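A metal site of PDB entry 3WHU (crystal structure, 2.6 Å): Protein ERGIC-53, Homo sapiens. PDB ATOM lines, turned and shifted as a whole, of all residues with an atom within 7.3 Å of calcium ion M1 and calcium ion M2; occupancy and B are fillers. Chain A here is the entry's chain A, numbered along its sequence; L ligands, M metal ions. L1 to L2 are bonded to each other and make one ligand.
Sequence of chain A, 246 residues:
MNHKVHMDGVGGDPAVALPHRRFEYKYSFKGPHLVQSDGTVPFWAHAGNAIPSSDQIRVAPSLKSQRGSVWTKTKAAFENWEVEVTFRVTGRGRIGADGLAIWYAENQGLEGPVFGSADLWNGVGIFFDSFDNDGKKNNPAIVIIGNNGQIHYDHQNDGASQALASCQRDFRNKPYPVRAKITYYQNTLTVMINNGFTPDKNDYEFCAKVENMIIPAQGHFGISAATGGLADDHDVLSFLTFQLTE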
ATOM      1  N   ASP A  98      -4.293  23.491  -5.527  1.00  0.00           N
ATOM      2  CA  ASP A  98      -3.635  24.251  -6.612  1.00  0.00           C
ATOM      3  C   ASP A  98      -2.314  23.597  -7.057  1.00  0.00           C
ATOM      4  O   ASP A  98      -1.910  23.711  -8.239  1.00  0.00           O
ATOM      5  CB  ASP A  98      -3.384  25.711  -6.200  1.00  0.00           C
ATOM      6  CG  ASP A  98      -3.977  26.707  -7.189  1.00  0.00           C
ATOM      7  OD1 ASP A  98      -4.141  27.887  -6.782  1.00  0.00           O
ATOM      8  OD2 ASP A  98      -4.287  26.339  -8.360  1.00  0.00           O
ATOM      9  N   GLY A  99      -1.650  22.921  -6.127  1.00  0.00           N
ATOM     10  CA  GLY A  99      -0.488  22.109  -6.437  1.00  0.00           C
ATOM     11  C   GLY A  99       0.652  22.329  -5.477  1.00  0.00           C
ATOM     12  O   GLY A  99       0.506  22.931  -4.392  1.00  0.00           O
ATOM     13  N   PHE A 115       2.711  28.950  -4.910  1.00  0.00           N
ATOM     14  CA  PHE A 115       2.346  27.676  -4.318  1.00  0.00           C
ATOM     15  C   PHE A 115       2.651  27.667  -2.815  1.00  0.00           C
ATOM     16  O   PHE A 115       3.394  26.815  -2.293  1.00  0.00           O
ATOM     17  CB  PHE A 115       3.063  26.562  -5.057  1.00  0.00           C
ATOM     18  CG  PHE A 115       2.539  26.357  -6.450  1.00  0.00           C
ATOM     19  CD1 PHE A 115       1.700  25.302  -6.742  1.00  0.00           C
ATOM     20  CD2 PHE A 115       2.868  27.240  -7.462  1.00  0.00           C
ATOM     21  CE1 PHE A 115       1.192  25.118  -8.002  1.00  0.00           C
ATOM     22  CE2 PHE A 115       2.371  27.052  -8.744  1.00  0.00           C
ATOM     23  CZ  PHE A 115       1.529  25.995  -9.015  1.00  0.00           C
ATOM     24  N   ASP A 129       1.693  21.336 -10.891  1.00  0.00           N
ATOM     25  CA  ASP A 129       0.588  22.273 -11.066  1.00  0.00           C
ATOM     26  C   ASP A 129      -0.682  21.544 -11.480  1.00  0.00           C
ATOM     27  O   ASP A 129      -0.834  21.100 -12.606  1.00  0.00           O
ATOM     28  CB  ASP A 129       0.980  23.324 -12.091  1.00  0.00           C
ATOM     29  CG  ASP A 129       0.053  24.508 -12.106  1.00  0.00           C
ATOM     30  OD1 ASP A 129      -1.142  24.360 -11.740  1.00  0.00           O
ATOM     31  OD2 ASP A 129       0.509  25.611 -12.514  1.00  0.00           O
ATOM     32  N   SER A 130      -1.603  21.434 -10.528  1.00  0.00           N
ATOM     33  CA  SER A 130      -2.804  20.650 -10.705  1.00  0.00           C
ATOM     34  C   SER A 130      -3.788  21.412 -11.565  1.00  0.00           C
ATOM     35  O   SER A 130      -4.658  20.816 -12.212  1.00  0.00           O
ATOM     36  CB  SER A 130      -3.444  20.350  -9.342  1.00  0.00           C
ATOM     37  OG  SER A 130      -2.489  20.209  -8.298  1.00  0.00           O
ATOM     38  N   PHE A 131      -3.678  22.746 -11.525  1.00  0.00           N
ATOM     39  CA  PHE A 131      -4.716  23.619 -12.064  1.00  0.00           C
ATOM     40  C   PHE A 131      -4.331  24.394 -13.333  1.00  0.00           C
ATOM     41  O   PHE A 131      -3.432  25.237 -13.328  1.00  0.00           O
ATOM     42  CB  PHE A 131      -5.256  24.575 -10.993  1.00  0.00           C
ATOM     43  CG  PHE A 131      -6.592  25.170 -11.370  1.00  0.00           C
ATOM     44  CD1 PHE A 131      -7.670  24.345 -11.697  1.00  0.00           C
ATOM     45  CD2 PHE A 131      -6.760  26.544 -11.451  1.00  0.00           C
ATOM     46  CE1 PHE A 131      -8.884  24.885 -12.071  1.00  0.00           C
ATOM     47  CE2 PHE A 131      -7.979  27.093 -11.848  1.00  0.00           C
ATOM     48  CZ  PHE A 131      -9.038  26.259 -12.146  1.00  0.00           C
ATOM     49  N   ASP A 132      -5.083  24.091 -14.391  1.00  0.00           N
ATOM     50  CA  ASP A 132      -4.924  24.721 -15.700  1.00  0.00           C
ATOM     51  C   ASP A 132      -5.404  26.206 -15.694  1.00  0.00           C
ATOM     52  O   ASP A 132      -6.503  26.507 -16.172  1.00  0.00           O
ATOM     53  CB  ASP A 132      -5.712  23.876 -16.731  1.00  0.00           C
ATOM     54  CG  ASP A 132      -5.410  24.238 -18.171  1.00  0.00           C
ATOM     55  OD1 ASP A 132      -4.233  24.521 -18.495  1.00  0.00           O
ATOM     56  OD2 ASP A 132      -6.367  24.222 -18.981  1.00  0.00           O
ATOM     57  N   ASN A 133      -4.594  27.119 -15.160  1.00  0.00           N
ATOM     58  CA  ASN A 133      -4.991  28.532 -14.982  1.00  0.00           C
ATOM     59  C   ASN A 133      -5.062  29.386 -16.275  1.00  0.00           C
ATOM     60  O   ASN A 133      -5.810  30.361 -16.346  1.00  0.00           O
ATOM     61  CB  ASN A 133      -4.053  29.259 -14.007  1.00  0.00           C
ATOM     62  CG  ASN A 133      -4.019  28.613 -12.629  1.00  0.00           C
ATOM     63  OD1 ASN A 133      -3.822  27.400 -12.505  1.00  0.00           O
ATOM     64  ND2 ASN A 133      -4.165  29.431 -11.585  1.00  0.00           N
ATOM     65  N   ASP A 134      -4.254  29.032 -17.266  1.00  0.00           N
ATOM     66  CA  ASP A 134      -4.263  29.710 -18.565  1.00  0.00           C
ATOM     67  C   ASP A 134      -4.906  28.789 -19.607  1.00  0.00           C
ATOM     68  O   ASP A 134      -4.361  28.588 -20.700  1.00  0.00           O
ATOM     69  CB  ASP A 134      -2.841  30.145 -18.974  1.00  0.00           C
ATOM     70  CG  ASP A 134      -1.820  28.996 -18.957  1.00  0.00           C
ATOM     71  OD1 ASP A 134      -2.199  27.838 -19.237  1.00  0.00           O
ATOM     72  OD2 ASP A 134      -0.640  29.242 -18.669  1.00  0.00           O
ATOM     73  N   GLY A 135      -6.057  28.210 -19.249  1.00  0.00           N
ATOM     74  CA  GLY A 135      -6.951  27.535 -20.199  1.00  0.00           C
ATOM     75  C   GLY A 135      -6.369  26.739 -21.358  1.00  0.00           C
ATOM     76  O   GLY A 135      -7.065  26.520 -22.331  1.00  0.00           O
ATOM     77  N   LYS A 136      -5.119  26.286 -21.241  1.00  0.00           N
ATOM     78  CA  LYS A 136      -4.425  25.578 -22.335  1.00  0.00           C
ATOM     79  C   LYS A 136      -4.619  24.051 -22.337  1.00  0.00           C
ATOM     80  O   LYS A 136      -3.930  23.370 -23.083  1.00  0.00           O
ATOM     81  CB  LYS A 136      -2.907  25.882 -22.300  1.00  0.00           C
ATOM     82  CG  LYS A 136      -2.454  27.150 -23.014  1.00  0.00           C
ATOM     83  CD  LYS A 136      -2.406  26.973 -24.528  1.00  0.00           C
ATOM     84  CE  LYS A 136      -2.061  28.285 -25.244  1.00  0.00           C
ATOM     85  NZ  LYS A 136      -2.438  28.317 -26.694  1.00  0.00           N
ATOM     86  N   LYS A 137      -5.520  23.495 -21.525  1.00  0.00           N
ATOM     87  CA  LYS A 137      -5.661  22.016 -21.438  1.00  0.00           C
ATOM     88  C   LYS A 137      -4.292  21.270 -21.353  1.00  0.00           C
ATOM     89  O   LYS A 137      -4.105  20.193 -21.940  1.00  0.00           O
ATOM     90  CB  LYS A 137      -6.472  21.485 -22.627  1.00  0.00           C
ATOM     91  CG  LYS A 137      -7.772  22.219 -22.946  1.00  0.00           C
ATOM     92  CD  LYS A 137      -8.349  21.718 -24.268  1.00  0.00           C
ATOM     93  CE  LYS A 137      -9.349  22.682 -24.886  1.00  0.00           C
ATOM     94  NZ  LYS A 137     -10.736  22.461 -24.428  1.00  0.00           N
ATOM     95  N   ASN A 138      -3.357  21.850 -20.611  1.00  0.00           N
ATOM     96  CA  ASN A 138      -1.981  21.362 -20.515  1.00  0.00           C
ATOM     97  C   ASN A 138      -1.570  20.933 -19.085  1.00  0.00           C
ATOM     98  O   ASN A 138      -0.374  20.871 -18.775  1.00  0.00           O
ATOM     99  CB  ASN A 138      -0.999  22.454 -21.014  1.00  0.00           C
ATOM    100  CG  ASN A 138      -1.185  23.783 -20.287  1.00  0.00           C
ATOM    101  OD1 ASN A 138      -2.275  24.076 -19.748  1.00  0.00           O
ATOM    102  ND2 ASN A 138      -0.143  24.594 -20.270  1.00  0.00           N
ATOM    103  N   ASN A 139      -2.580  20.653 -18.233  1.00  0.00           N
ATOM    104  CA  ASN A 139      -2.368  20.344 -16.805  1.00  0.00           C
ATOM    105  C   ASN A 139      -3.061  19.036 -16.400  1.00  0.00           C
ATOM    106  O   ASN A 139      -4.018  18.632 -17.055  1.00  0.00           O
ATOM    107  CB  ASN A 139      -2.886  21.495 -15.925  1.00  0.00           C
ATOM    108  CG  ASN A 139      -1.919  22.670 -15.852  1.00  0.00           C
ATOM    109  OD1 ASN A 139      -1.240  23.005 -16.830  1.00  0.00           O
ATOM    110  ND2 ASN A 139      -1.862  23.311 -14.699  1.00  0.00           N
ATOM    111  N   ALA A 141       0.782  19.396 -14.488  1.00  0.00           N
ATOM    112  CA  ALA A 141       2.048  19.626 -15.172  1.00  0.00           C
ATOM    113  C   ALA A 141       3.195  19.980 -14.257  1.00  0.00           C
ATOM    114  O   ALA A 141       3.023  20.688 -13.261  1.00  0.00           O
ATOM    115  CB  ALA A 141       1.874  20.734 -16.186  1.00  0.00           C
ATOM    116  N   TYR A 153       6.281  35.196 -10.342  1.00  0.00           N
ATOM    117  CA  TYR A 153       5.700  33.965 -10.894  1.00  0.00           C
ATOM    118  C   TYR A 153       4.306  34.224 -11.511  1.00  0.00           C
ATOM    119  O   TYR A 153       3.415  34.786 -10.852  1.00  0.00           O
ATOM    120  CB  TYR A 153       5.662  32.806  -9.861  1.00  0.00           C
ATOM    121  CG  TYR A 153       4.711  31.725 -10.283  1.00  0.00           C
ATOM    122  CD1 TYR A 153       4.970  30.963 -11.416  1.00  0.00           C
ATOM    123  CD2 TYR A 153       3.524  31.513  -9.601  1.00  0.00           C
ATOM    124  CE1 TYR A 153       4.076  29.983 -11.841  1.00  0.00           C
ATOM    125  CE2 TYR A 153       2.624  30.541 -10.013  1.00  0.00           C
ATOM    126  CZ  TYR A 153       2.904  29.772 -11.139  1.00  0.00           C
ATOM    127  OH  TYR A 153       1.996  28.806 -11.551  1.00  0.00           O
ATOM    128  N   ASP A 154       4.136  33.805 -12.767  1.00  0.00           N
ATOM    129  CA  ASP A 154       2.944  34.148 -13.513  1.00  0.00           C
ATOM    130  C   ASP A 154       1.851  33.170 -13.189  1.00  0.00           C
ATOM    131  O   ASP A 154       1.483  32.331 -14.018  1.00  0.00           O
ATOM    132  CB  ASP A 154       3.227  34.205 -15.020  1.00  0.00           C
ATOM    133  CG  ASP A 154       2.298  35.192 -15.741  1.00  0.00           C
ATOM    134  OD1 ASP A 154       1.062  35.165 -15.500  1.00  0.00           O
ATOM    135  OD2 ASP A 154       2.801  35.989 -16.545  1.00  0.00           O
ATOM    136  N   HIS A 155       1.313  33.303 -11.982  1.00  0.00           N
ATOM    137  CA  HIS A 155       0.329  32.363 -11.473  1.00  0.00           C
ATOM    138  C   HIS A 155      -0.714  32.056 -12.511  1.00  0.00           C
ATOM    139  O   HIS A 155      -0.862  30.908 -12.900  1.00  0.00           O
ATOM    140  CB  HIS A 155      -0.349  32.845 -10.188  1.00  0.00           C
ATOM    141  CG  HIS A 155      -1.098  31.768  -9.470  1.00  0.00           C
ATOM    142  ND1 HIS A 155      -0.574  31.081  -8.390  1.00  0.00           N
ATOM    143  CD2 HIS A 155      -2.313  31.216  -9.710  1.00  0.00           C
ATOM    144  CE1 HIS A 155      -1.448  30.178  -7.982  1.00  0.00           C
ATOM    145  NE2 HIS A 155      -2.512  30.239  -8.763  1.00  0.00           N
ATOM    146  N   GLN A 156      -1.402  33.099 -12.975  1.00  0.00           N
ATOM    147  CA  GLN A 156      -2.503  32.941 -13.933  1.00  0.00           C
ATOM    148  C   GLN A 156      -2.064  32.284 -15.231  1.00  0.00           C
ATOM    149  O   GLN A 156      -2.886  31.667 -15.915  1.00  0.00           O
ATOM    150  CB  GLN A 156      -3.180  34.281 -14.212  1.00  0.00           C
ATOM    151  CG  GLN A 156      -4.192  34.671 -13.149  1.00  0.00           C
ATOM    152  CD  GLN A 156      -3.940  36.071 -12.608  1.00  0.00           C
ATOM    153  OE1 GLN A 156      -2.856  36.344 -12.078  1.00  0.00           O
ATOM    154  NE2 GLN A 156      -4.926  36.963 -12.739  1.00  0.00           N
ATOM    155  N   ASN A 157      -0.782  32.411 -15.568  1.00  0.00           N
ATOM    156  CA  ASN A 157      -0.236  31.727 -16.744  1.00  0.00           C
ATOM    157  C   ASN A 157       0.672  30.524 -16.438  1.00  0.00           C
ATOM    158  O   ASN A 157       1.486  30.148 -17.291  1.00  0.00           O
ATOM    159  CB  ASN A 157       0.492  32.713 -17.671  1.00  0.00           C
ATOM    160  CG  ASN A 157      -0.466  33.556 -18.486  1.00  0.00           C
ATOM    161  OD1 ASN A 157      -1.194  33.033 -19.333  1.00  0.00           O
ATOM    162  ND2 ASN A 157      -0.476  34.856 -18.236  1.00  0.00           N
ATOM    163  N   ASP A 158       0.521  29.918 -15.262  1.00  0.00           N
ATOM    164  CA  ASP A 158       1.229  28.679 -14.948  1.00  0.00           C
ATOM    165  C   ASP A 158       2.697  28.794 -15.364  1.00  0.00           C
ATOM    166  O   ASP A 158       3.245  27.884 -15.984  1.00  0.00           O
ATOM    167  CB  ASP A 158       0.576  27.499 -15.693  1.00  0.00           C
ATOM    168  CG  ASP A 158      -0.840  27.183 -15.177  1.00  0.00           C
ATOM    169  OD1 ASP A 158      -1.094  27.405 -13.972  1.00  0.00           O
ATOM    170  OD2 ASP A 158      -1.688  26.689 -15.967  1.00  0.00           O
ATOM    171  N   GLY A 159       3.303  29.945 -15.055  1.00  0.00           N
ATOM    172  CA  GLY A 159       4.655  30.310 -15.499  1.00  0.00           C
ATOM    173  C   GLY A 159       5.146  29.916 -16.899  1.00  0.00           C
ATOM    174  O   GLY A 159       6.358  29.883 -17.123  1.00  0.00           O
ATOM    175  N   ALA A 160       4.242  29.651 -17.847  1.00  0.00           N
ATOM    176  CA  ALA A 160       4.627  29.008 -19.114  1.00  0.00           C
ATOM    177  C   ALA A 160       5.788  29.735 -19.806  1.00  0.00           C
ATOM    178  O   ALA A 160       6.689  29.107 -20.336  1.00  0.00           O
ATOM    179  CB  ALA A 160       3.425  28.838 -20.039  1.00  0.00           C
ATOM    180  N   GLN A 168       4.539  17.003 -18.675  1.00  0.00           N
ATOM    181  CA  GLN A 168       3.136  16.840 -18.366  1.00  0.00           C
ATOM    182  C   GLN A 168       2.810  15.457 -17.879  1.00  0.00           C
ATOM    183  O   GLN A 168       2.448  14.593 -18.669  1.00  0.00           O
ATOM    184  CB  GLN A 168       2.282  17.147 -19.604  1.00  0.00           C
ATOM    185  CG  GLN A 168       1.819  18.603 -19.718  1.00  0.00           C
ATOM    186  CD  GLN A 168       0.664  18.802 -20.700  1.00  0.00           C
ATOM    187  OE1 GLN A 168       0.661  19.773 -21.449  1.00  0.00           O
ATOM    188  NE2 GLN A 168      -0.312  17.898 -20.676  1.00  0.00           N
HETATM  189  C1  LIG L   1      -9.457  30.416  -8.167  1.00  0.00           C
HETATM  190  C2  LIG L   1      -8.142  31.226  -8.083  1.00  0.00           C
HETATM  191  C3  LIG L   1      -6.941  30.629  -8.788  1.00  0.00           C
HETATM  192  C4  LIG L   1      -6.864  29.133  -8.483  1.00  0.00           C
HETATM  193  C5  LIG L   1      -8.192  28.400  -8.654  1.00  0.00           C
HETATM  194  C6  LIG L   1      -8.114  27.002  -8.046  1.00  0.00           C
HETATM  195  O1  LIG L   1     -10.136  30.636  -9.383  1.00  0.00           O
HETATM  196  O2  LIG L   1      -7.676  31.393  -6.752  1.00  0.00           O
HETATM  197  O3  LIG L   1      -5.788  31.297  -8.277  1.00  0.00           O
HETATM  198  O4  LIG L   1      -5.900  28.547  -9.331  1.00  0.00           O
HETATM  199  O5  LIG L   1      -9.287  29.014  -8.025  1.00  0.00           O
HETATM  200  O6  LIG L   1      -8.003  27.103  -6.623  1.00  0.00           O
HETATM  201  C1  LG2 L   2      -7.840  32.745  -6.373  1.00  0.00           C
HETATM  202  C2  LG2 L   2      -7.259  33.081  -4.981  1.00  0.00           C
HETATM  203  C3  LG2 L   2      -8.125  32.476  -3.845  1.00  0.00           C
HETATM  204  C4  LG2 L   2      -9.571  32.959  -4.076  1.00  0.00           C
HETATM  205  C5  LG2 L   2     -10.020  32.344  -5.425  1.00  0.00           C
HETATM  206  C6  LG2 L   2     -11.524  32.475  -5.743  1.00  0.00           C
HETATM  207  O1  LG2 L   2      -7.130  34.515  -4.876  1.00  0.00           O
HETATM  208  O2  LG2 L   2      -7.686  32.797  -2.516  1.00  0.00           O
HETATM  209  O3  LG2 L   2     -10.385  32.634  -2.958  1.00  0.00           O
HETATM  210  O4  LG2 L   2      -9.240  32.939  -6.459  1.00  0.00           O
HETATM  211  O5  LG2 L   2     -11.828  33.856  -5.899  1.00  0.00           O
HETATM  212 CA    CA M   1      -1.793  26.839 -11.954  1.00  0.00          CA
HETATM  213 CA    CA M   2      -1.179  25.874 -17.940  1.00  0.00          CA
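OD2 of Asp 158 binds calcium ion M2, at 2.2 Å. Calcium ion M2 is bound by OD1 of Asp 134. OD1 of Asn 138 is bound to calcium ion M2 (2.8 Å). Calcium ion M2 is bound by the side-chain amide nitrogen (ND2) of Asn 138, at 2.9 Å. Calcium ion M2 has four donor atoms within binding distance. Slightly farther from calcium ion M2 lies the side-chain amide oxygen (OD1) of Asn 139 (3.1 Å).
Asp 132 touches calcium ion M2. Of the 24 residues printed, 5 come within 4 Å of calcium ion M2.
A ring nitrogen (NE2) of His 155 sits close to the side-chain amide nitrogen of Asn 133, at 3.4 Å. The side-chain carboxylate (OD2) of Asp 134 lies close to the backbone carbonyl oxygen (O) of Asn 157, at 2.7 Å. N of Asp 134 is in hydrogen-bond range of O of Gln 156. O of Asp 129 sits at hydrogen-bond distance from ND2 of Asn 139 (3.2 Å). N of Asp 129 sits at hydrogen-bond distance from O of Ala 141. The backbone carbonyl oxygen of Phe 131 sits close to the side-chain amide nitrogen of Asn 139. O of Asn 138 sits close to OE1 of Gln 168, 3.1 Å away. The side-chain amide nitrogen (ND2) of Asn 139 lies close to the backbone NH (N) of Asp 132 (3.3 Å).
Along chain A the residues within 4 Å of calcium ion M1 span positions 129 to 158.
OD1 of Asn 133 is bound to calcium ion M1 (2.2 Å). Calcium ion M1 is bound by the side-chain carboxylate (OD1) of Asp 158. OD1 of Asp 129 binds calcium ion M1 (2.6 Å). OD2 of Asp 129 is bound to calcium ion M1. O of Phe 131 is bound to calcium ion M1 (2.7 Å).
The side-chain amide nitrogen of Asn 133 lies within hydrogen-bond range of an oxygen (O4) of LIG L1 (3.0 Å). An oxygen (O3) of LIG L1 sits at hydrogen-bond distance from a ring nitrogen (NE2) of His 155, at 3.5 Å. The side-chain carboxylate (OD2) of Asp 98 sits at hydrogen-bond distance from an oxygen (O4) of LIG L1, 2.9 Å away.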
